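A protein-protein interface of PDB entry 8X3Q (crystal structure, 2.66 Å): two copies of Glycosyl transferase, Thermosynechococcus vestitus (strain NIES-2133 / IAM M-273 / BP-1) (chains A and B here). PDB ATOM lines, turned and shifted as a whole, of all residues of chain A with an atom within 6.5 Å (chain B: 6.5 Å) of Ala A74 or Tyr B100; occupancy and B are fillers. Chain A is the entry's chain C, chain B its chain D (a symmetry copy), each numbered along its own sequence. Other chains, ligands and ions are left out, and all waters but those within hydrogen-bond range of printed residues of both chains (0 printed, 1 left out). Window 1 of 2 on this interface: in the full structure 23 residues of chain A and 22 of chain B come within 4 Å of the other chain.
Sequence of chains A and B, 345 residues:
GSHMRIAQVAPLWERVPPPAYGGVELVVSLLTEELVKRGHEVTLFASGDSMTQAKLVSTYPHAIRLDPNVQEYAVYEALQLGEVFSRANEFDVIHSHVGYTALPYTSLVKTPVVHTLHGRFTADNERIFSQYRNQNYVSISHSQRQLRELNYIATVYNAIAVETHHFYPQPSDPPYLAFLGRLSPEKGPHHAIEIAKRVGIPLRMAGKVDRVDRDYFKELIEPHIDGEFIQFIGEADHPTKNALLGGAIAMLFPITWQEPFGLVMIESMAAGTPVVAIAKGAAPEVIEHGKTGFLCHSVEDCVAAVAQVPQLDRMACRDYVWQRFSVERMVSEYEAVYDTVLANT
Among the printed residues, pairs that only touch across the chains: Val A75 with Tyr B100, Val A75 with Ile B128, Leu A79 with Ile B128, Ala A78 with Pro B104, Ala A74 with Tyr B100, Glu A72 with Tyr B100, Ala A78 with Ile B128 and Val A75 with Asn B125.
Ala A74 touches just one residue of chain B: Tyr B100 (3.7 Å). Tyr B100 touches three residues of chain A. Of the printed residues of chain B, Ala A78 touches Pro B104 (3.7 Å) and Ile B128 (3.9 Å). Of the printed residues of chain B, Glu A72 touches Tyr B100. Of the printed residues of chain B, Val A75 touches Tyr B100 (3.5 Å), Asn B125 (3.99 Å) and Ile B128 (3.6 Å). Printed residues of chain A within 4 Å of Pro B104: Ala A78 (3.7 Å). Of the printed residues of chain A, Ile B128 touches Val A75 (3.6 Å), Ala A78 (3.9 Å) and Leu A79 (3.7 Å). The nearest residue of chain A that does not touch Tyr B100 is Ala A78 (4.7 Å).
Of the 10 printed residues of chain A, 5 touch a printed residue of chain B. Printed residues of chain A that touch a printed residue of chain B: Glu A72, Ala A74, Val A75, Ala A78 and Leu A79.
No position is printed for both chains.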
ATOM      1  N   TRP A  13      -7.044  36.091 -22.031  1.00  0.00           N
ATOM      2  CA  TRP A  13      -8.440  35.893 -22.403  1.00  0.00           C
ATOM      3  C   TRP A  13      -9.066  37.176 -22.930  1.00  0.00           C
ATOM      4  O   TRP A  13      -9.930  37.127 -23.812  1.00  0.00           O
ATOM      5  CB  TRP A  13      -9.232  35.364 -21.207  1.00  0.00           C
ATOM      6  CG  TRP A  13      -8.870  33.964 -20.831  1.00  0.00           C
ATOM      7  CD1 TRP A  13      -8.140  33.568 -19.747  1.00  0.00           C
ATOM      8  CD2 TRP A  13      -9.212  32.770 -21.543  1.00  0.00           C
ATOM      9  NE1 TRP A  13      -8.011  32.200 -19.740  1.00  0.00           N
ATOM     10  CE2 TRP A  13      -8.660  31.686 -20.832  1.00  0.00           C
ATOM     11  CE3 TRP A  13      -9.934  32.513 -22.713  1.00  0.00           C
ATOM     12  CZ2 TRP A  13      -8.807  30.365 -21.252  1.00  0.00           C
ATOM     13  CZ3 TRP A  13     -10.079  31.201 -23.129  1.00  0.00           C
ATOM     14  CH2 TRP A  13      -9.519  30.144 -22.400  1.00  0.00           C
ATOM     15  N   GLN A  71      -7.937  27.257 -30.176  1.00  0.00           N
ATOM     16  CA  GLN A  71      -8.491  26.180 -29.370  1.00  0.00           C
ATOM     17  C   GLN A  71      -7.652  25.851 -28.141  1.00  0.00           C
ATOM     18  O   GLN A  71      -8.144  25.154 -27.244  1.00  0.00           O
ATOM     19  CB  GLN A  71      -8.654  24.908 -30.217  1.00  0.00           C
ATOM     20  CG  GLN A  71      -9.938  24.847 -31.034  1.00  0.00           C
ATOM     21  CD  GLN A  71      -9.865  25.671 -32.305  1.00  0.00           C
ATOM     22  OE1 GLN A  71      -8.867  25.638 -33.024  1.00  0.00           O
ATOM     23  NE2 GLN A  71     -10.928  26.415 -32.589  1.00  0.00           N
ATOM     24  N   GLU A  72      -6.414  26.339 -28.070  1.00  0.00           N
ATOM     25  CA  GLU A  72      -5.477  26.008 -26.996  1.00  0.00           C
ATOM     26  C   GLU A  72      -4.936  27.308 -26.405  1.00  0.00           C
ATOM     27  O   GLU A  72      -3.933  27.846 -26.882  1.00  0.00           O
ATOM     28  CB  GLU A  72      -4.357  25.111 -27.516  1.00  0.00           C
ATOM     29  CG  GLU A  72      -4.799  23.688 -27.827  1.00  0.00           C
ATOM     30  CD  GLU A  72      -3.747  22.902 -28.584  1.00  0.00           C
ATOM     31  OE1 GLU A  72      -3.726  22.980 -29.831  1.00  0.00           O
ATOM     32  OE2 GLU A  72      -2.942  22.205 -27.931  1.00  0.00           O
ATOM     33  N   TYR A  73      -5.611  27.811 -25.368  1.00  0.00           N
ATOM     34  CA  TYR A  73      -5.145  29.021 -24.698  1.00  0.00           C
ATOM     35  C   TYR A  73      -3.781  28.810 -24.050  1.00  0.00           C
ATOM     36  O   TYR A  73      -2.947  29.723 -24.036  1.00  0.00           O
ATOM     37  CB  TYR A  73      -6.181  29.461 -23.658  1.00  0.00           C
ATOM     38  CG  TYR A  73      -5.719  30.545 -22.703  1.00  0.00           C
ATOM     39  CD1 TYR A  73      -5.081  30.225 -21.509  1.00  0.00           C
ATOM     40  CD2 TYR A  73      -5.940  31.887 -22.987  1.00  0.00           C
ATOM     41  CE1 TYR A  73      -4.663  31.210 -20.634  1.00  0.00           C
ATOM     42  CE2 TYR A  73      -5.527  32.880 -22.114  1.00  0.00           C
ATOM     43  CZ  TYR A  73      -4.890  32.534 -20.940  1.00  0.00           C
ATOM     44  OH  TYR A  73      -4.476  33.514 -20.066  1.00  0.00           O
ATOM     45  N   ALA A  74      -3.532  27.609 -23.519  1.00  0.00           N
ATOM     46  CA  ALA A  74      -2.297  27.353 -22.784  1.00  0.00           C
ATOM     47  C   ALA A  74      -1.055  27.508 -23.653  1.00  0.00           C
ATOM     48  O   ALA A  74       0.029  27.774 -23.119  1.00  0.00           O
ATOM     49  CB  ALA A  74      -2.333  25.954 -22.169  1.00  0.00           C
ATOM     50  N   VAL A  75      -1.186  27.354 -24.972  1.00  0.00           N
ATOM     51  CA  VAL A  75      -0.032  27.477 -25.861  1.00  0.00           C
ATOM     52  C   VAL A  75       0.534  28.890 -25.796  1.00  0.00           C
ATOM     53  O   VAL A  75       1.748  29.092 -25.668  1.00  0.00           O
ATOM     54  CB  VAL A  75      -0.420  27.091 -27.299  1.00  0.00           C
ATOM     55  CG1 VAL A  75       0.684  27.466 -28.272  1.00  0.00           C
ATOM     56  CG2 VAL A  75      -0.731  25.606 -27.386  1.00  0.00           C
ATOM     57  N   TYR A  76      -0.342  29.890 -25.888  1.00  0.00           N
ATOM     58  CA  TYR A  76       0.096  31.279 -25.872  1.00  0.00           C
ATOM     59  C   TYR A  76       0.376  31.759 -24.455  1.00  0.00           C
ATOM     60  O   TYR A  76       1.179  32.679 -24.260  1.00  0.00           O
ATOM     61  CB  TYR A  76      -0.954  32.151 -26.560  1.00  0.00           C
ATOM     62  CG  TYR A  76      -1.307  31.626 -27.933  1.00  0.00           C
ATOM     63  CD1 TYR A  76      -0.536  31.956 -29.040  1.00  0.00           C
ATOM     64  CD2 TYR A  76      -2.388  30.772 -28.117  1.00  0.00           C
ATOM     65  CE1 TYR A  76      -0.844  31.467 -30.296  1.00  0.00           C
ATOM     66  CE2 TYR A  76      -2.702  30.278 -29.369  1.00  0.00           C
ATOM     67  CZ  TYR A  76      -1.927  30.629 -30.454  1.00  0.00           C
ATOM     68  OH  TYR A  76      -2.234  30.141 -31.704  1.00  0.00           O
ATOM     69  N   GLU A  77      -0.279  31.152 -23.465  1.00  0.00           N
ATOM     70  CA  GLU A  77       0.055  31.414 -22.071  1.00  0.00           C
ATOM     71  C   GLU A  77       1.496  31.012 -21.771  1.00  0.00           C
ATOM     72  O   GLU A  77       2.243  31.763 -21.131  1.00  0.00           O
ATOM     73  CB  GLU A  77      -0.923  30.664 -21.163  1.00  0.00           C
ATOM     74  CG  GLU A  77      -0.675  30.810 -19.673  1.00  0.00           C
ATOM     75  CD  GLU A  77      -1.730  30.095 -18.846  1.00  0.00           C
ATOM     76  OE1 GLU A  77      -2.453  30.770 -18.085  1.00  0.00           O
ATOM     77  OE2 GLU A  77      -1.842  28.857 -18.969  1.00  0.00           O
ATOM     78  N   ALA A  78       1.902  29.820 -22.224  1.00  0.00           N
ATOM     79  CA  ALA A  78       3.280  29.377 -22.030  1.00  0.00           C
ATOM     80  C   ALA A  78       4.275  30.210 -22.830  1.00  0.00           C
ATOM     81  O   ALA A  78       5.408  30.415 -22.379  1.00  0.00           O
ATOM     82  CB  ALA A  78       3.410  27.899 -22.403  1.00  0.00           C
ATOM     83  N   LEU A  79       3.878  30.687 -24.012  1.00  0.00           N
ATOM     84  CA  LEU A  79       4.762  31.530 -24.815  1.00  0.00           C
ATOM     85  C   LEU A  79       5.119  32.807 -24.068  1.00  0.00           C
ATOM     86  O   LEU A  79       6.294  33.177 -23.958  1.00  0.00           O
ATOM     87  CB  LEU A  79       4.105  31.858 -26.156  1.00  0.00           C
ATOM     88  CG  LEU A  79       4.264  30.843 -27.291  1.00  0.00           C
ATOM     89  CD1 LEU A  79       3.277  31.140 -28.408  1.00  0.00           C
ATOM     90  CD2 LEU A  79       5.691  30.848 -27.816  1.00  0.00           C
ATOM     91  N   VAL B  98       5.716  15.670 -21.799  1.00  0.00           N
ATOM     92  CA  VAL B  98       4.521  16.417 -21.423  1.00  0.00           C
ATOM     93  C   VAL B  98       4.179  17.509 -22.433  1.00  0.00           C
ATOM     94  O   VAL B  98       3.268  18.307 -22.189  1.00  0.00           O
ATOM     95  CB  VAL B  98       4.665  17.008 -20.011  1.00  0.00           C
ATOM     96  CG1 VAL B  98       5.069  15.924 -19.022  1.00  0.00           C
ATOM     97  CG2 VAL B  98       5.679  18.144 -20.010  1.00  0.00           C
ATOM     98  N   GLY B  99       4.877  17.562 -23.563  1.00  0.00           N
ATOM     99  CA  GLY B  99       4.521  18.494 -24.613  1.00  0.00           C
ATOM    100  C   GLY B  99       5.108  19.884 -24.479  1.00  0.00           C
ATOM    101  O   GLY B  99       6.176  20.069 -23.888  1.00  0.00           O
ATOM    102  N   TYR B 100       4.395  20.873 -25.022  1.00  0.00           N
ATOM    103  CA  TYR B 100       4.935  22.222 -25.167  1.00  0.00           C
ATOM    104  C   TYR B 100       5.069  22.961 -23.842  1.00  0.00           C
ATOM    105  O   TYR B 100       5.790  23.962 -23.782  1.00  0.00           O
ATOM    106  CB  TYR B 100       4.051  23.031 -26.121  1.00  0.00           C
ATOM    107  CG  TYR B 100       2.591  23.092 -25.716  1.00  0.00           C
ATOM    108  CD1 TYR B 100       2.141  24.037 -24.801  1.00  0.00           C
ATOM    109  CD2 TYR B 100       1.664  22.207 -26.251  1.00  0.00           C
ATOM    110  CE1 TYR B 100       0.810  24.097 -24.429  1.00  0.00           C
ATOM    111  CE2 TYR B 100       0.330  22.258 -25.884  1.00  0.00           C
ATOM    112  CZ  TYR B 100      -0.090  23.206 -24.972  1.00  0.00           C
ATOM    113  OH  TYR B 100      -1.414  23.267 -24.603  1.00  0.00           O
ATOM    114  N   THR B 101       4.384  22.510 -22.788  1.00  0.00           N
ATOM    115  CA  THR B 101       4.441  23.208 -21.507  1.00  0.00           C
ATOM    116  C   THR B 101       5.840  23.223 -20.902  1.00  0.00           C
ATOM    117  O   THR B 101       6.088  23.991 -19.968  1.00  0.00           O
ATOM    118  CB  THR B 101       3.460  22.584 -20.512  1.00  0.00           C
ATOM    119  OG1 THR B 101       3.919  21.282 -20.134  1.00  0.00           O
ATOM    120  CG2 THR B 101       2.077  22.467 -21.137  1.00  0.00           C
ATOM    121  N   ALA B 102       6.757  22.391 -21.397  1.00  0.00           N
ATOM    122  CA  ALA B 102       8.117  22.346 -20.876  1.00  0.00           C
ATOM    123  C   ALA B 102       9.107  23.180 -21.681  1.00  0.00           C
ATOM    124  O   ALA B 102      10.225  23.408 -21.204  1.00  0.00           O
ATOM    125  CB  ALA B 102       8.611  20.895 -20.812  1.00  0.00           C
ATOM    126  N   LEU B 103       8.729  23.643 -22.874  1.00  0.00           N
ATOM    127  CA  LEU B 103       9.657  24.405 -23.708  1.00  0.00           C
ATOM    128  C   LEU B 103      10.151  25.685 -23.045  1.00  0.00           C
ATOM    129  O   LEU B 103      11.371  25.931 -23.070  1.00  0.00           O
ATOM    130  CB  LEU B 103       9.015  24.691 -25.070  1.00  0.00           C
ATOM    131  CG  LEU B 103       8.409  23.483 -25.784  1.00  0.00           C
ATOM    132  CD1 LEU B 103       7.822  23.903 -27.117  1.00  0.00           C
ATOM    133  CD2 LEU B 103       9.450  22.393 -25.973  1.00  0.00           C
ATOM    134  N   PRO B 104       9.303  26.540 -22.459  1.00  0.00           N
ATOM    135  CA  PRO B 104       9.833  27.767 -21.838  1.00  0.00           C
ATOM    136  C   PRO B 104      10.789  27.504 -20.685  1.00  0.00           C
ATOM    137  O   PRO B 104      11.567  28.399 -20.331  1.00  0.00           O
ATOM    138  CB  PRO B 104       8.572  28.502 -21.361  1.00  0.00           C
ATOM    139  CG  PRO B 104       7.481  27.490 -21.395  1.00  0.00           C
ATOM    140  CD  PRO B 104       7.830  26.545 -22.485  1.00  0.00           C
ATOM    141  N   ASN B 125      -0.418  24.976 -31.586  1.00  0.00           N
ATOM    142  CA  ASN B 125       0.829  24.531 -30.969  1.00  0.00           C
ATOM    143  C   ASN B 125       2.035  24.674 -31.891  1.00  0.00           C
ATOM    144  O   ASN B 125       3.170  24.643 -31.409  1.00  0.00           O
ATOM    145  CB  ASN B 125       0.692  23.084 -30.461  1.00  0.00           C
ATOM    146  CG  ASN B 125       0.760  22.029 -31.571  1.00  0.00           C
ATOM    147  OD1 ASN B 125       0.912  22.331 -32.755  1.00  0.00           O
ATOM    148  ND2 ASN B 125       0.645  20.768 -31.170  1.00  0.00           N
ATOM    149  N   ILE B 128       4.234  27.747 -30.784  1.00  0.00           N
ATOM    150  CA  ILE B 128       5.145  27.672 -29.645  1.00  0.00           C
ATOM    151  C   ILE B 128       6.354  26.803 -29.975  1.00  0.00           C
ATOM    152  O   ILE B 128       7.472  27.086 -29.533  1.00  0.00           O
ATOM    153  CB  ILE B 128       4.413  27.174 -28.384  1.00  0.00           C
ATOM    154  CG1 ILE B 128       5.350  27.235 -27.173  1.00  0.00           C
ATOM    155  CG2 ILE B 128       3.880  25.762 -28.572  1.00  0.00           C
ATOM    156  CD1 ILE B 128       4.748  26.695 -25.897  1.00  0.00           C
ATOM    157  N   PHE B 129       6.157  25.740 -30.757  1.00  0.00           N
ATOM    158  CA  PHE B 129       7.295  24.949 -31.210  1.00  0.00           C
ATOM    159  C   PHE B 129       8.182  25.764 -32.140  1.00  0.00           C
ATOM    160  O   PHE B 129       9.408  25.587 -32.146  1.00  0.00           O
ATOM    161  CB  PHE B 129       6.812  23.672 -31.909  1.00  0.00           C
ATOM    162  CG  PHE B 129       6.298  22.611 -30.967  1.00  0.00           C
ATOM    163  CD1 PHE B 129       7.133  22.031 -30.025  1.00  0.00           C
ATOM    164  CD2 PHE B 129       4.980  22.189 -31.031  1.00  0.00           C
ATOM    165  CE1 PHE B 129       6.660  21.052 -29.163  1.00  0.00           C
ATOM    166  CE2 PHE B 129       4.500  21.214 -30.174  1.00  0.00           C
ATOM    167  CZ  PHE B 129       5.343  20.644 -29.238  1.00  0.00           C
ATOM    168  N   TYR B 132      10.685  27.791 -30.345  1.00  0.00           N
ATOM    169  CA  TYR B 132      11.671  26.910 -29.736  1.00  0.00           C
ATOM    170  C   TYR B 132      12.106  25.850 -30.739  1.00  0.00           C
ATOM    171  O   TYR B 132      12.235  24.668 -30.417  1.00  0.00           O
ATOM    172  CB  TYR B 132      11.115  26.277 -28.458  1.00  0.00           C
ATOM    173  CG  TYR B 132      10.750  27.285 -27.386  1.00  0.00           C
ATOM    174  CD1 TYR B 132      11.729  27.895 -26.614  1.00  0.00           C
ATOM    175  CD2 TYR B 132       9.422  27.624 -27.147  1.00  0.00           C
ATOM    176  CE1 TYR B 132      11.396  28.818 -25.634  1.00  0.00           C
ATOM    177  CE2 TYR B 132       9.082  28.544 -26.169  1.00  0.00           C
ATOM    178  CZ  TYR B 132      10.072  29.137 -25.417  1.00  0.00           C
ATOM    179  OH  TYR B 132       9.740  30.052 -24.444  1.00  0.00           O
